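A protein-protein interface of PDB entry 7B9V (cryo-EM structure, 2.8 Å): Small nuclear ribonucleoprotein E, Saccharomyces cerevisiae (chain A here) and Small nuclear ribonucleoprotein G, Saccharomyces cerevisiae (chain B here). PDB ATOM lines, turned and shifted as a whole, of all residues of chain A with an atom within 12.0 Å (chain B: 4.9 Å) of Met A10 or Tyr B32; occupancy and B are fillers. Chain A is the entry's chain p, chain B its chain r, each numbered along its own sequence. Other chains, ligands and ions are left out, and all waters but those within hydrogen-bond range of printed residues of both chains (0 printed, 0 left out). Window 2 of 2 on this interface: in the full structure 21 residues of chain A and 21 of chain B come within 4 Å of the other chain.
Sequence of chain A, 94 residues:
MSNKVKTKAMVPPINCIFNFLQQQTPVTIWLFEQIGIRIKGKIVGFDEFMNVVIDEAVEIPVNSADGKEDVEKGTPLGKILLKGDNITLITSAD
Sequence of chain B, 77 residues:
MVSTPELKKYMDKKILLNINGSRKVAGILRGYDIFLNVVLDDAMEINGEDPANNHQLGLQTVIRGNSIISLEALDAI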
ATOM      1  N   MET A  10      26.894   6.953 -18.487  1.00  0.00           N
ATOM      2  CA  MET A  10      26.658   6.307 -17.206  1.00  0.00           C
ATOM      3  C   MET A  10      27.051   7.210 -16.046  1.00  0.00           C
ATOM      4  O   MET A  10      28.219   7.579 -15.902  1.00  0.00           O
ATOM      5  CB  MET A  10      27.432   4.991 -17.120  1.00  0.00           C
ATOM      6  CG  MET A  10      27.253   4.246 -15.809  1.00  0.00           C
ATOM      7  SD  MET A  10      25.541   3.790 -15.485  1.00  0.00           S
ATOM      8  CE  MET A  10      25.345   2.437 -16.646  1.00  0.00           C
ATOM      9  N   VAL A  11      26.068   7.567 -15.230  1.00  0.00           N
ATOM     10  CA  VAL A  11      26.290   8.356 -14.020  1.00  0.00           C
ATOM     11  C   VAL A  11      25.888   7.491 -12.830  1.00  0.00           C
ATOM     12  O   VAL A  11      24.710   7.119 -12.748  1.00  0.00           O
ATOM     13  CB  VAL A  11      25.477   9.660 -14.040  1.00  0.00           C
ATOM     14  CG1 VAL A  11      25.736  10.472 -12.770  1.00  0.00           C
ATOM     15  CG2 VAL A  11      25.776  10.476 -15.289  1.00  0.00           C
ATOM     16  N   PRO A  12      26.825   7.027 -12.008  1.00  0.00           N
ATOM     17  CA  PRO A  12      26.443   6.335 -10.772  1.00  0.00           C
ATOM     18  C   PRO A  12      25.604   7.226  -9.892  1.00  0.00           C
ATOM     19  O   PRO A  12      25.759   8.465  -9.885  1.00  0.00           O
ATOM     20  CB  PRO A  12      27.792   6.017 -10.118  1.00  0.00           C
ATOM     21  CG  PRO A  12      28.701   5.822 -11.276  1.00  0.00           C
ATOM     22  CD  PRO A  12      28.253   6.826 -12.316  1.00  0.00           C
ATOM     23  N   PRO A  13      24.655   6.642  -9.131  1.00  0.00           N
ATOM     24  CA  PRO A  13      23.694   7.461  -8.367  1.00  0.00           C
ATOM     25  C   PRO A  13      24.313   8.303  -7.260  1.00  0.00           C
ATOM     26  O   PRO A  13      23.899   9.456  -7.061  1.00  0.00           O
ATOM     27  CB  PRO A  13      22.695   6.423  -7.785  1.00  0.00           C
ATOM     28  CG  PRO A  13      22.773   5.266  -8.713  1.00  0.00           C
ATOM     29  CD  PRO A  13      24.260   5.246  -9.096  1.00  0.00           C
ATOM     30  N   ILE A  14      25.265   7.734  -6.506  1.00  0.00           N
ATOM     31  CA  ILE A  14      25.956   8.467  -5.445  1.00  0.00           C
ATOM     32  C   ILE A  14      26.762   9.634  -6.012  1.00  0.00           C
ATOM     33  O   ILE A  14      26.905  10.682  -5.365  1.00  0.00           O
ATOM     34  CB  ILE A  14      26.788   7.491  -4.572  1.00  0.00           C
ATOM     35  CG1 ILE A  14      28.010   6.909  -5.294  1.00  0.00           C
ATOM     36  CG2 ILE A  14      25.904   6.373  -4.032  1.00  0.00           C
ATOM     37  CD1 ILE A  14      28.886   6.038  -4.420  1.00  0.00           C
ATOM     38  N   ASN A  15      27.309   9.475  -7.226  1.00  0.00           N
ATOM     39  CA  ASN A  15      27.984  10.572  -7.910  1.00  0.00           C
ATOM     40  C   ASN A  15      27.017  11.682  -8.286  1.00  0.00           C
ATOM     41  O   ASN A  15      27.383  12.862  -8.256  1.00  0.00           O
ATOM     42  CB  ASN A  15      28.722  10.072  -9.153  1.00  0.00           C
ATOM     43  CG  ASN A  15      29.874   9.158  -8.812  1.00  0.00           C
ATOM     44  OD1 ASN A  15      29.982   8.683  -7.685  1.00  0.00           O
ATOM     45  ND2 ASN A  15      30.748   8.909  -9.783  1.00  0.00           N
ATOM     46  N   CYS A  16      25.781  11.333  -8.678  1.00  0.00           N
ATOM     47  CA  CYS A  16      24.764  12.365  -8.863  1.00  0.00           C
ATOM     48  C   CYS A  16      24.401  13.077  -7.566  1.00  0.00           C
ATOM     49  O   CYS A  16      24.195  14.302  -7.588  1.00  0.00           O
ATOM     50  CB  CYS A  16      23.510  11.771  -9.505  1.00  0.00           C
ATOM     51  SG  CYS A  16      22.273  13.039  -9.916  1.00  0.00           S
ATOM     52  N   ILE A  17      24.302  12.338  -6.439  1.00  0.00           N
ATOM     53  CA  ILE A  17      24.104  12.968  -5.117  1.00  0.00           C
ATOM     54  C   ILE A  17      25.224  13.974  -4.831  1.00  0.00           C
ATOM     55  O   ILE A  17      24.978  15.098  -4.353  1.00  0.00           O
ATOM     56  CB  ILE A  17      23.957  11.907  -4.001  1.00  0.00           C
ATOM     57  CG1 ILE A  17      22.801  10.942  -4.288  1.00  0.00           C
ATOM     58  CG2 ILE A  17      23.670  12.559  -2.656  1.00  0.00           C
ATOM     59  CD1 ILE A  17      22.741   9.708  -3.362  1.00  0.00           C
ATOM     60  N   ASN A  19      27.049  15.503  -7.122  1.00  0.00           N
ATOM     61  CA  ASN A  19      26.768  16.617  -8.035  1.00  0.00           C
ATOM     62  C   ASN A  19      25.582  17.486  -7.621  1.00  0.00           C
ATOM     63  O   ASN A  19      25.416  18.576  -8.189  1.00  0.00           O
ATOM     64  CB  ASN A  19      26.533  16.116  -9.460  1.00  0.00           C
ATOM     65  CG  ASN A  19      27.823  15.700 -10.148  1.00  0.00           C
ATOM     66  OD1 ASN A  19      28.851  15.535  -9.505  1.00  0.00           O
ATOM     67  ND2 ASN A  19      27.764  15.541 -11.462  1.00  0.00           N
ATOM     68  N   MET A  50      23.424   6.835   2.379  1.00  0.00           N
ATOM     69  CA  MET A  50      22.478   7.826   1.838  1.00  0.00           C
ATOM     70  C   MET A  50      21.759   8.666   2.928  1.00  0.00           C
ATOM     71  O   MET A  50      20.671   9.209   2.710  1.00  0.00           O
ATOM     72  CB  MET A  50      21.523   7.126   0.834  1.00  0.00           C
ATOM     73  CG  MET A  50      20.727   7.994  -0.185  1.00  0.00           C
ATOM     74  SD  MET A  50      19.963   7.138  -1.551  1.00  0.00           S
ATOM     75  CE  MET A  50      19.103   8.528  -2.278  1.00  0.00           C
ATOM     76  N   PRO B   5      21.784  -6.716 -10.720  1.00  0.00           N
ATOM     77  CA  PRO B   5      20.901  -5.668 -11.203  1.00  0.00           C
ATOM     78  C   PRO B   5      21.031  -5.387 -12.716  1.00  0.00           C
ATOM     79  O   PRO B   5      21.831  -4.544 -13.142  1.00  0.00           O
ATOM     80  CB  PRO B   5      21.350  -4.488 -10.373  1.00  0.00           C
ATOM     81  CG  PRO B   5      22.823  -4.761  -9.976  1.00  0.00           C
ATOM     82  CD  PRO B   5      23.137  -6.179 -10.462  1.00  0.00           C
ATOM     83  N   LEU B   7      19.818  -3.952 -15.260  1.00  0.00           N
ATOM     84  CA  LEU B   7      19.290  -2.723 -15.848  1.00  0.00           C
ATOM     85  C   LEU B   7      20.051  -2.239 -17.077  1.00  0.00           C
ATOM     86  O   LEU B   7      19.558  -1.314 -17.734  1.00  0.00           O
ATOM     87  CB  LEU B   7      19.221  -1.611 -14.787  1.00  0.00           C
ATOM     88  CG  LEU B   7      18.192  -1.526 -13.642  1.00  0.00           C
ATOM     89  CD1 LEU B   7      16.827  -1.437 -14.246  1.00  0.00           C
ATOM     90  CD2 LEU B   7      18.148  -2.703 -12.733  1.00  0.00           C
ATOM     91  N   LYS B   8      21.263  -2.768 -17.340  1.00  0.00           N
ATOM     92  CA  LYS B   8      22.104  -2.388 -18.492  1.00  0.00           C
ATOM     93  C   LYS B   8      21.374  -2.483 -19.837  1.00  0.00           C
ATOM     94  O   LYS B   8      21.631  -1.702 -20.762  1.00  0.00           O
ATOM     95  CB  LYS B   8      23.353  -3.271 -18.510  1.00  0.00           C
ATOM     96  CG  LYS B   8      24.418  -2.859 -19.509  1.00  0.00           C
ATOM     97  CD  LYS B   8      25.687  -3.682 -19.403  1.00  0.00           C
ATOM     98  CE  LYS B   8      26.678  -3.226 -20.462  1.00  0.00           C
ATOM     99  NZ  LYS B   8      27.934  -4.013 -20.420  1.00  0.00           N
ATOM    100  N   ARG B  30      19.248   7.170 -16.418  1.00  0.00           N
ATOM    101  CA  ARG B  30      20.662   7.493 -16.611  1.00  0.00           C
ATOM    102  C   ARG B  30      21.638   6.514 -15.951  1.00  0.00           C
ATOM    103  O   ARG B  30      22.674   6.182 -16.540  1.00  0.00           O
ATOM    104  CB  ARG B  30      20.946   8.924 -16.174  1.00  0.00           C
ATOM    105  CG  ARG B  30      20.172   9.981 -16.973  1.00  0.00           C
ATOM    106  CD  ARG B  30      20.380   9.911 -18.499  1.00  0.00           C
ATOM    107  NE  ARG B  30      19.803  11.093 -19.144  1.00  0.00           N
ATOM    108  CZ  ARG B  30      19.688  11.289 -20.450  1.00  0.00           C
ATOM    109  NH1 ARG B  30      20.064  10.368 -21.325  1.00  0.00           N
ATOM    110  NH2 ARG B  30      19.155  12.430 -20.888  1.00  0.00           N
ATOM    111  N   GLY B  31      21.341   6.030 -14.744  1.00  0.00           N
ATOM    112  CA  GLY B  31      22.267   5.132 -14.066  1.00  0.00           C
ATOM    113  C   GLY B  31      21.654   4.443 -12.863  1.00  0.00           C
ATOM    114  O   GLY B  31      20.559   4.788 -12.414  1.00  0.00           O
ATOM    115  N   TYR B  32      22.399   3.459 -12.350  1.00  0.00           N
ATOM    116  CA  TYR B  32      21.933   2.580 -11.279  1.00  0.00           C
ATOM    117  C   TYR B  32      23.113   1.996 -10.504  1.00  0.00           C
ATOM    118  O   TYR B  32      24.258   2.041 -10.963  1.00  0.00           O
ATOM    119  CB  TYR B  32      21.094   1.442 -11.902  1.00  0.00           C
ATOM    120  CG  TYR B  32      21.923   0.576 -12.867  1.00  0.00           C
ATOM    121  CD1 TYR B  32      22.010   0.911 -14.219  1.00  0.00           C
ATOM    122  CD2 TYR B  32      22.562  -0.595 -12.434  1.00  0.00           C
ATOM    123  CE1 TYR B  32      22.744   0.144 -15.089  1.00  0.00           C
ATOM    124  CE2 TYR B  32      23.311  -1.344 -13.293  1.00  0.00           C
ATOM    125  CZ  TYR B  32      23.386  -0.981 -14.619  1.00  0.00           C
ATOM    126  OH  TYR B  32      24.157  -1.737 -15.456  1.00  0.00           O
ATOM    127  N   ASP B  33      22.824   1.422  -9.320  1.00  0.00           N
ATOM    128  CA  ASP B  33      23.845   0.749  -8.516  1.00  0.00           C
ATOM    129  C   ASP B  33      23.268  -0.514  -7.872  1.00  0.00           C
ATOM    130  O   ASP B  33      22.140  -0.916  -8.162  1.00  0.00           O
ATOM    131  CB  ASP B  33      24.448   1.734  -7.484  1.00  0.00           C
ATOM    132  CG  ASP B  33      23.433   2.296  -6.444  1.00  0.00           C
ATOM    133  OD1 ASP B  33      22.323   1.755  -6.212  1.00  0.00           O
ATOM    134  OD2 ASP B  33      23.769   3.343  -5.849  1.00  0.00           O
ATOM    135  N   ILE B  34      24.100  -1.166  -7.037  1.00  0.00           N
ATOM    136  CA  ILE B  34      23.791  -2.483  -6.460  1.00  0.00           C
ATOM    137  C   ILE B  34      22.548  -2.459  -5.560  1.00  0.00           C
ATOM    138  O   ILE B  34      21.781  -3.433  -5.515  1.00  0.00           O
ATOM    139  CB  ILE B  34      25.049  -3.016  -5.722  1.00  0.00           C
ATOM    140  CG1 ILE B  34      26.208  -3.219  -6.697  1.00  0.00           C
ATOM    141  CG2 ILE B  34      24.826  -4.343  -4.965  1.00  0.00           C
ATOM    142  CD1 ILE B  34      25.878  -4.140  -7.864  1.00  0.00           C
ATOM    143  N   ASN B  37      19.545   2.012  -6.328  1.00  0.00           N
ATOM    144  CA  ASN B  37      19.320   3.441  -6.466  1.00  0.00           C
ATOM    145  C   ASN B  37      19.305   3.756  -7.951  1.00  0.00           C
ATOM    146  O   ASN B  37      20.136   3.266  -8.704  1.00  0.00           O
ATOM    147  CB  ASN B  37      20.402   4.276  -5.774  1.00  0.00           C
ATOM    148  CG  ASN B  37      20.574   3.940  -4.286  1.00  0.00           C
ATOM    149  OD1 ASN B  37      19.610   3.820  -3.537  1.00  0.00           O
ATOM    150  ND2 ASN B  37      21.825   3.784  -3.869  1.00  0.00           N
ATOM    151  N   VAL B  38      18.345   4.563  -8.374  1.00  0.00           N
ATOM    152  CA  VAL B  38      18.183   4.868  -9.785  1.00  0.00           C
ATOM    153  C   VAL B  38      18.247   6.372  -9.966  1.00  0.00           C
ATOM    154  O   VAL B  38      17.526   7.113  -9.289  1.00  0.00           O
ATOM    155  CB  VAL B  38      16.860   4.255 -10.298  1.00  0.00           C
ATOM    156  CG1 VAL B  38      16.211   5.044 -11.420  1.00  0.00           C
ATOM    157  CG2 VAL B  38      17.114   2.827 -10.777  1.00  0.00           C
ATOM    158  N   VAL B  39      19.102   6.817 -10.877  1.00  0.00           N
ATOM    159  CA  VAL B  39      19.128   8.200 -11.316  1.00  0.00           C
ATOM    160  C   VAL B  39      18.524   8.285 -12.715  1.00  0.00           C
ATOM    161  O   VAL B  39      18.846   7.481 -13.603  1.00  0.00           O
ATOM    162  CB  VAL B  39      20.532   8.828 -11.189  1.00  0.00           C
ATOM    163  CG1 VAL B  39      21.578   8.194 -12.081  1.00  0.00           C
ATOM    164  CG2 VAL B  39      20.453  10.305 -11.486  1.00  0.00           C
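O of Val B39 is in hydrogen-bond range of N of Arg B30.
The backbone carbonyl oxygen of Gly B31 sits at hydrogen-bond distance from the backbone NH of Val B39 (2.9 Å).
N of Asn B37 lies within hydrogen-bond range of OD1 of Asp B33.
Hydrophobic or aromatic side chains of chain A within 4 Å of the printed part of chain B: Met A10, Pro A13 and Met A50.
Of the 11 printed residues of chain B, 6 touch a printed residue of chain A.
Hydrophobic or aromatic side chains of chain B within 4 Å of the printed part of chain A: Tyr B32 and Val B39.
Along chain B the printed residues that touch a printed residue of chain A span positions 30 to 39.
Among the printed residues, 11 pairs touch across the chains.
Of the printed residues of chain B, Met A10 touches Arg B30 (3.9 Å), Gly B31 (3.8 Å) and Tyr B32 (3.8 Å).
Of the printed residues of chain A, Tyr B32 touches Met A10 (3.8 Å) and Pro A13 (3.7 Å).
No residue of chain A comes within 4 Å of Pro B5.
Gly B31 touches just these residues of chain A: Met A10 (3.8 Å) and Val A11 (3.4 Å).
Of chain A, only Pro A13 comes within 4 Å of Asp B33.
Of the printed residues of chain B, Pro A13 touches Tyr B32 (3.7 Å), Asp B33 (3.6 Å) and Asn B37 (3.3 Å).
Of the printed residues of chain A, Asn B37 touches Pro A13 (3.3 Å) and Met A50 (3.9 Å).
Of the printed residues of chain B, Cys A16 touches Val B39 (3.6 Å).
Of the printed residues of chain B, Met A50 touches Asn B37.
Printed residues of chain B within 4 Å of Val A11: Arg B30 (3.9 Å), Gly B31 (3.4 Å) and Val B39 (3.4 Å).
The nearest residue of chain A that does not touch Tyr B32 is Val A11 (4.3 Å).
Arg B30 touches Met A10 (O to SD, 3.9 Å).
SD of Met A10 touches CA of Gly B31, 3.8 Å away.
Met A10 touches Tyr B32.
Val A11 touches Gly B31.
Val A11 touches Val B39 (O to CG1, 3.4 Å).
CD of Pro A13 touches O of Tyr B32, 3.7 Å away.
Asp B33 touches Pro A13.
Asn B37 touches Pro A13 (O to CG, 3.3 Å).
Cys A16 touches Val B39 (SG to CG2, 3.6 Å).
Asn B37 touches Met A50.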
